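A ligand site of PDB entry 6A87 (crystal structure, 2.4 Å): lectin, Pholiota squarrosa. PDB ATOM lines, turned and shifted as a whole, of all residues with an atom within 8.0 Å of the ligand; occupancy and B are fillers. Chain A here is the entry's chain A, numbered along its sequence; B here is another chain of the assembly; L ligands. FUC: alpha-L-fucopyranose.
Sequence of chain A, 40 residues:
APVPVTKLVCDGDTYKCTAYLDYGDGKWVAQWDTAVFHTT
The backbone NH of Gly 12 sits at hydrogen-bond distance from an oxygen (O4) of the ligand (3.2 Å). An oxygen (O4) of the ligand is in hydrogen-bond range of the backbone carbonyl oxygen (O) of Ala 1 of chain B. OD1 of Asp 13 lies within hydrogen-bond range of O2 of the ligand. N of Ala 1 of chain B sits at hydrogen-bond distance from O3 of the ligand, 2.8 Å away.
The backbone carbonyl oxygen of Trp 28 of chain B is in hydrogen-bond range of the backbone NH of Leu 21 of chain B (3.0 Å). N of Ala 1 of chain B is in hydrogen-bond range of OD1 of Asp 11 (2.7 Å). The side-chain carboxylate of Asp 11 lies within hydrogen-bond range of the backbone NH of Asp 13 (2.9 Å). The side-chain carboxylate (OD2) of Asp 13 is in hydrogen-bond range of the backbone NH (N) of Ala 1 of chain B (3.0 Å).
Residues that only touch the ligand: Tyr 23 of chain B and Leu 21 of chain B. Hydrophobic or aromatic side chains within 4 Å of the ligand: Ala 1 of chain B, Leu 21 of chain B and Tyr 23 of chain B. Of the 22 residues printed, 5 come within 4 Å of the ligand. Along chain A the residues within 4 Å of the ligand span positions 12 to 13. The nearest printed residue that does not touch the ligand is Val 3 of chain B (4.03 Å).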
ATOM      1  N   CYS A  10      15.329 -16.098 -17.487  1.00  0.00           N
ATOM      2  CA  CYS A  10      13.988 -16.229 -16.978  1.00  0.00           C
ATOM      3  C   CYS A  10      13.046 -16.680 -18.113  1.00  0.00           C
ATOM      4  O   CYS A  10      13.296 -16.475 -19.300  1.00  0.00           O
ATOM      5  CB  CYS A  10      13.502 -14.950 -16.308  1.00  0.00           C
ATOM      6  SG  CYS A  10      14.656 -14.328 -15.054  1.00  0.00           S
ATOM      7  N   ASP A  11      11.968 -17.329 -17.678  1.00  0.00           N
ATOM      8  CA  ASP A  11      11.022 -17.980 -18.529  1.00  0.00           C
ATOM      9  C   ASP A  11       9.621 -17.486 -18.155  1.00  0.00           C
ATOM     10  O   ASP A  11       9.161 -17.707 -17.036  1.00  0.00           O
ATOM     11  CB  ASP A  11      11.135 -19.488 -18.343  1.00  0.00           C
ATOM     12  CG  ASP A  11      10.440 -20.297 -19.423  1.00  0.00           C
ATOM     13  OD1 ASP A  11       9.448 -19.777 -19.999  1.00  0.00           O
ATOM     14  OD2 ASP A  11      10.904 -21.411 -19.693  1.00  0.00           O
ATOM     15  N   GLY A  12       8.960 -16.820 -19.113  1.00  0.00           N
ATOM     16  CA  GLY A  12       7.583 -16.308 -18.939  1.00  0.00           C
ATOM     17  C   GLY A  12       6.513 -17.390 -19.030  1.00  0.00           C
ATOM     18  O   GLY A  12       5.375 -17.175 -18.615  1.00  0.00           O
ATOM     19  N   ASP A  13       6.855 -18.556 -19.590  1.00  0.00           N
ATOM     20  CA  ASP A  13       5.915 -19.668 -19.606  1.00  0.00           C
ATOM     21  C   ASP A  13       5.860 -20.265 -18.205  1.00  0.00           C
ATOM     22  O   ASP A  13       4.772 -20.450 -17.670  1.00  0.00           O
ATOM     23  CB  ASP A  13       6.286 -20.720 -20.653  1.00  0.00           C
ATOM     24  CG  ASP A  13       6.261 -20.191 -22.077  1.00  0.00           C
ATOM     25  OD1 ASP A  13       5.428 -19.290 -22.351  1.00  0.00           O
ATOM     26  OD2 ASP A  13       7.090 -20.654 -22.897  1.00  0.00           O
ATOM     27  N   THR A  14       7.038 -20.533 -17.617  1.00  0.00           N
ATOM     28  CA  THR A  14       7.141 -21.225 -16.337  1.00  0.00           C
ATOM     29  C   THR A  14       7.102 -20.238 -15.155  1.00  0.00           C
ATOM     30  O   THR A  14       6.844 -20.648 -14.046  1.00  0.00           O
ATOM     31  CB  THR A  14       8.384 -22.118 -16.257  1.00  0.00           C
ATOM     32  OG1 THR A  14       9.546 -21.300 -16.232  1.00  0.00           O
ATOM     33  CG2 THR A  14       8.489 -23.116 -17.403  1.00  0.00           C
ATOM     34  N   TYR A  15       7.341 -18.959 -15.384  1.00  0.00           N
ATOM     35  CA  TYR A  15       7.462 -17.985 -14.297  1.00  0.00           C
ATOM     36  C   TYR A  15       8.573 -18.416 -13.333  1.00  0.00           C
ATOM     37  O   TYR A  15       8.450 -18.298 -12.134  1.00  0.00           O
ATOM     38  CB  TYR A  15       6.085 -17.776 -13.642  1.00  0.00           C
ATOM     39  CG  TYR A  15       5.098 -17.069 -14.552  1.00  0.00           C
ATOM     40  CD1 TYR A  15       4.319 -17.783 -15.444  1.00  0.00           C
ATOM     41  CD2 TYR A  15       5.007 -15.690 -14.566  1.00  0.00           C
ATOM     42  CE1 TYR A  15       3.440 -17.146 -16.319  1.00  0.00           C
ATOM     43  CE2 TYR A  15       4.139 -15.033 -15.422  1.00  0.00           C
ATOM     44  CZ  TYR A  15       3.355 -15.766 -16.303  1.00  0.00           C
ATOM     45  OH  TYR A  15       2.526 -15.127 -17.164  1.00  0.00           O
ATOM     46  N   LYS A  16       9.685 -18.918 -13.894  1.00  0.00           N
ATOM     47  CA  LYS A  16      10.906 -19.258 -13.147  1.00  0.00           C
ATOM     48  C   LYS A  16      12.103 -18.451 -13.671  1.00  0.00           C
ATOM     49  O   LYS A  16      12.241 -18.257 -14.878  1.00  0.00           O
ATOM     50  CB  LYS A  16      11.255 -20.732 -13.314  1.00  0.00           C
ATOM     51  CG  LYS A  16      10.172 -21.718 -12.909  1.00  0.00           C
ATOM     52  CD  LYS A  16       9.813 -21.626 -11.448  1.00  0.00           C
ATOM     53  CE  LYS A  16       9.242 -22.899 -10.857  1.00  0.00           C
ATOM     54  NZ  LYS A  16       9.312 -22.854  -9.375  1.00  0.00           N
ATOM     55  N   VAL A  36       6.856 -12.056 -14.303  1.00  0.00           N
ATOM     56  CA  VAL A  36       7.339 -11.694 -15.599  1.00  0.00           C
ATOM     57  C   VAL A  36       6.243 -10.886 -16.264  1.00  0.00           C
ATOM     58  O   VAL A  36       5.090 -11.287 -16.254  1.00  0.00           O
ATOM     59  CB  VAL A  36       7.653 -12.911 -16.480  1.00  0.00           C
ATOM     60  CG1 VAL A  36       8.177 -12.468 -17.828  1.00  0.00           C
ATOM     61  CG2 VAL A  36       8.629 -13.882 -15.826  1.00  0.00           C
ATOM     62  N   PHE A  37       6.626  -9.784 -16.901  1.00  0.00           N
ATOM     63  CA  PHE A  37       5.657  -8.936 -17.537  1.00  0.00           C
ATOM     64  C   PHE A  37       6.342  -7.869 -18.396  1.00  0.00           C
ATOM     65  O   PHE A  37       7.525  -7.535 -18.208  1.00  0.00           O
ATOM     66  CB  PHE A  37       4.768  -8.268 -16.483  1.00  0.00           C
ATOM     67  CG  PHE A  37       5.485  -7.425 -15.454  1.00  0.00           C
ATOM     68  CD1 PHE A  37       5.877  -7.969 -14.247  1.00  0.00           C
ATOM     69  CD2 PHE A  37       5.684  -6.077 -15.671  1.00  0.00           C
ATOM     70  CE1 PHE A  37       6.487  -7.180 -13.274  1.00  0.00           C
ATOM     71  CE2 PHE A  37       6.294  -5.288 -14.699  1.00  0.00           C
ATOM     72  CZ  PHE A  37       6.696  -5.846 -13.510  1.00  0.00           C
ATOM     73  N   HIS A  38       5.555  -7.405 -19.373  1.00  0.00           N
ATOM     74  CA  HIS A  38       5.870  -6.291 -20.229  1.00  0.00           C
ATOM     75  C   HIS A  38       5.666  -5.017 -19.432  1.00  0.00           C
ATOM     76  O   HIS A  38       4.602  -4.829 -18.887  1.00  0.00           O
ATOM     77  CB  HIS A  38       4.932  -6.237 -21.435  1.00  0.00           C
ATOM     78  CG  HIS A  38       5.353  -5.273 -22.483  1.00  0.00           C
ATOM     79  ND1 HIS A  38       4.923  -3.955 -22.495  1.00  0.00           N
ATOM     80  CD2 HIS A  38       6.128  -5.444 -23.568  1.00  0.00           C
ATOM     81  CE1 HIS A  38       5.434  -3.354 -23.552  1.00  0.00           C
ATOM     82  NE2 HIS A  38       6.182  -4.253 -24.232  1.00  0.00           N
ATOM     83  N   ALA B   1       9.867 -19.568 -22.630  1.00  0.00           N
ATOM     84  CA  ALA B   1      11.207 -20.203 -22.749  1.00  0.00           C
ATOM     85  C   ALA B   1      12.262 -19.325 -22.073  1.00  0.00           C
ATOM     86  O   ALA B   1      12.063 -18.112 -21.926  1.00  0.00           O
ATOM     87  CB  ALA B   1      11.557 -20.394 -24.204  1.00  0.00           C
ATOM     88  N   PRO B   2      13.414 -19.912 -21.679  1.00  0.00           N
ATOM     89  CA  PRO B   2      14.434 -19.159 -20.979  1.00  0.00           C
ATOM     90  C   PRO B   2      14.956 -18.121 -21.992  1.00  0.00           C
ATOM     91  O   PRO B   2      15.256 -18.472 -23.130  1.00  0.00           O
ATOM     92  CB  PRO B   2      15.495 -20.176 -20.536  1.00  0.00           C
ATOM     93  CG  PRO B   2      14.960 -21.542 -20.952  1.00  0.00           C
ATOM     94  CD  PRO B   2      13.827 -21.301 -21.926  1.00  0.00           C
ATOM     95  N   VAL B   3      14.972 -16.863 -21.577  1.00  0.00           N
ATOM     96  CA  VAL B   3      15.643 -15.797 -22.296  1.00  0.00           C
ATOM     97  C   VAL B   3      16.621 -15.126 -21.333  1.00  0.00           C
ATOM     98  O   VAL B   3      16.353 -15.073 -20.123  1.00  0.00           O
ATOM     99  CB  VAL B   3      14.649 -14.780 -22.894  1.00  0.00           C
ATOM    100  CG1 VAL B   3      13.703 -15.447 -23.875  1.00  0.00           C
ATOM    101  CG2 VAL B   3      13.875 -14.031 -21.825  1.00  0.00           C
ATOM    102  N   PRO B   4      17.755 -14.613 -21.855  1.00  0.00           N
ATOM    103  CA  PRO B   4      18.818 -14.066 -21.027  1.00  0.00           C
ATOM    104  C   PRO B   4      18.347 -12.855 -20.220  1.00  0.00           C
ATOM    105  O   PRO B   4      17.555 -12.072 -20.704  1.00  0.00           O
ATOM    106  CB  PRO B   4      19.891 -13.605 -22.034  1.00  0.00           C
ATOM    107  CG  PRO B   4      19.609 -14.425 -23.276  1.00  0.00           C
ATOM    108  CD  PRO B   4      18.101 -14.539 -23.297  1.00  0.00           C
ATOM    109  N   LEU B  21      15.129  -8.342 -19.501  1.00  0.00           N
ATOM    110  CA  LEU B  21      15.187  -9.540 -20.326  1.00  0.00           C
ATOM    111  C   LEU B  21      15.506  -9.218 -21.786  1.00  0.00           C
ATOM    112  O   LEU B  21      15.029  -8.262 -22.353  1.00  0.00           O
ATOM    113  CB  LEU B  21      13.847 -10.260 -20.243  1.00  0.00           C
ATOM    114  CG  LEU B  21      13.406 -10.665 -18.839  1.00  0.00           C
ATOM    115  CD1 LEU B  21      12.135 -11.496 -18.924  1.00  0.00           C
ATOM    116  CD2 LEU B  21      14.503 -11.419 -18.098  1.00  0.00           C
ATOM    117  N   ASP B  22      16.314 -10.073 -22.373  1.00  0.00           N
ATOM    118  CA  ASP B  22      16.609 -10.028 -23.777  1.00  0.00           C
ATOM    119  C   ASP B  22      15.481 -10.734 -24.541  1.00  0.00           C
ATOM    120  O   ASP B  22      15.561 -11.930 -24.790  1.00  0.00           O
ATOM    121  CB  ASP B  22      17.961 -10.683 -24.055  1.00  0.00           C
ATOM    122  CG  ASP B  22      18.348 -10.545 -25.497  1.00  0.00           C
ATOM    123  OD1 ASP B  22      17.563  -9.928 -26.231  1.00  0.00           O
ATOM    124  OD2 ASP B  22      19.454 -11.016 -25.849  1.00  0.00           O
ATOM    125  N   TYR B  23      14.429  -9.988 -24.845  1.00  0.00           N
ATOM    126  CA  TYR B  23      13.300 -10.480 -25.622  1.00  0.00           C
ATOM    127  C   TYR B  23      12.460  -9.305 -26.156  1.00  0.00           C
ATOM    128  O   TYR B  23      12.260  -8.301 -25.472  1.00  0.00           O
ATOM    129  CB  TYR B  23      12.424 -11.433 -24.798  1.00  0.00           C
ATOM    130  CG  TYR B  23      11.263 -11.991 -25.584  1.00  0.00           C
ATOM    131  CD1 TYR B  23      11.475 -12.605 -26.813  1.00  0.00           C
ATOM    132  CD2 TYR B  23       9.945 -11.865 -25.149  1.00  0.00           C
ATOM    133  CE1 TYR B  23      10.437 -13.093 -27.572  1.00  0.00           C
ATOM    134  CE2 TYR B  23       8.893 -12.360 -25.899  1.00  0.00           C
ATOM    135  CZ  TYR B  23       9.136 -12.969 -27.116  1.00  0.00           C
ATOM    136  OH  TYR B  23       8.119 -13.451 -27.884  1.00  0.00           O
ATOM    137  N   GLY B  24      11.957  -9.453 -27.380  1.00  0.00           N
ATOM    138  CA  GLY B  24      10.881  -8.621 -27.893  1.00  0.00           C
ATOM    139  C   GLY B  24      11.304  -7.167 -28.016  1.00  0.00           C
ATOM    140  O   GLY B  24      12.389  -6.896 -28.477  1.00  0.00           O
ATOM    141  N   LYS B  27      11.203  -4.380 -23.350  1.00  0.00           N
ATOM    142  CA  LYS B  27      10.509  -3.853 -22.149  1.00  0.00           C
ATOM    143  C   LYS B  27      10.013  -4.983 -21.248  1.00  0.00           C
ATOM    144  O   LYS B  27       9.189  -4.792 -20.360  1.00  0.00           O
ATOM    145  CB  LYS B  27       9.343  -2.959 -22.574  1.00  0.00           C
ATOM    146  CG  LYS B  27       9.737  -1.544 -22.989  1.00  0.00           C
ATOM    147  CD  LYS B  27       8.621  -0.814 -23.680  1.00  0.00           C
ATOM    148  CE  LYS B  27       8.459   0.620 -23.222  1.00  0.00           C
ATOM    149  NZ  LYS B  27       7.060   1.089 -23.400  1.00  0.00           N
ATOM    150  N   TRP B  28      10.506  -6.191 -21.469  1.00  0.00           N
ATOM    151  CA  TRP B  28      10.133  -7.284 -20.610  1.00  0.00           C
ATOM    152  C   TRP B  28      11.091  -7.352 -19.421  1.00  0.00           C
ATOM    153  O   TRP B  28      12.303  -7.234 -19.589  1.00  0.00           O
ATOM    154  CB  TRP B  28      10.131  -8.572 -21.415  1.00  0.00           C
ATOM    155  CG  TRP B  28       9.058  -8.609 -22.457  1.00  0.00           C
ATOM    156  CD1 TRP B  28       9.141  -8.206 -23.762  1.00  0.00           C
ATOM    157  CD2 TRP B  28       7.727  -9.113 -22.286  1.00  0.00           C
ATOM    158  NE1 TRP B  28       7.956  -8.418 -24.411  1.00  0.00           N
ATOM    159  CE2 TRP B  28       7.070  -8.990 -23.531  1.00  0.00           C
ATOM    160  CE3 TRP B  28       7.028  -9.669 -21.208  1.00  0.00           C
ATOM    161  CZ2 TRP B  28       5.744  -9.389 -23.718  1.00  0.00           C
ATOM    162  CZ3 TRP B  28       5.721 -10.071 -21.394  1.00  0.00           C
ATOM    163  CH2 TRP B  28       5.089  -9.923 -22.638  1.00  0.00           C
ATOM    164  N   VAL B  29      10.530  -7.582 -18.231  1.00  0.00           N
ATOM    165  CA  VAL B  29      11.309  -7.729 -17.033  1.00  0.00           C
ATOM    166  C   VAL B  29      10.744  -8.891 -16.207  1.00  0.00           C
ATOM    167  O   VAL B  29       9.652  -9.375 -16.448  1.00  0.00           O
ATOM    168  CB  VAL B  29      11.286  -6.445 -16.190  1.00  0.00           C
ATOM    169  CG1 VAL B  29      11.754  -5.222 -16.958  1.00  0.00           C
ATOM    170  CG2 VAL B  29       9.896  -6.227 -15.597  1.00  0.00           C
ATOM    171  N   ALA B  30      11.501  -9.255 -15.169  1.00  0.00           N
ATOM    172  CA  ALA B  30      11.111 -10.219 -14.218  1.00  0.00           C
ATOM    173  C   ALA B  30      11.371  -9.622 -12.844  1.00  0.00           C
ATOM    174  O   ALA B  30      12.321  -8.892 -12.691  1.00  0.00           O
ATOM    175  CB  ALA B  30      11.888 -11.488 -14.430  1.00  0.00           C
HETATM  176  C1  FUC L   1       6.774 -14.801 -22.087  1.00  0.00           C
HETATM  177  C2  FUC L   1       7.278 -16.104 -22.773  1.00  0.00           C
HETATM  178  C3  FUC L   1       8.523 -15.956 -23.705  1.00  0.00           C
HETATM  179  C4  FUC L   1       9.612 -15.114 -23.024  1.00  0.00           C
HETATM  180  C5  FUC L   1       8.956 -13.831 -22.480  1.00  0.00           C
HETATM  181  C6  FUC L   1       9.993 -12.940 -21.807  1.00  0.00           C
HETATM  182  O1  FUC L   1       6.062 -13.931 -23.001  1.00  0.00           O
HETATM  183  O2  FUC L   1       6.130 -16.650 -23.458  1.00  0.00           O
HETATM  184  O3  FUC L   1       9.103 -17.256 -24.033  1.00  0.00           O
HETATM  185  O4  FUC L   1      10.142 -15.934 -21.948  1.00  0.00           O
HETATM  186  O5  FUC L   1       7.946 -14.172 -21.485  1.00  0.00           O
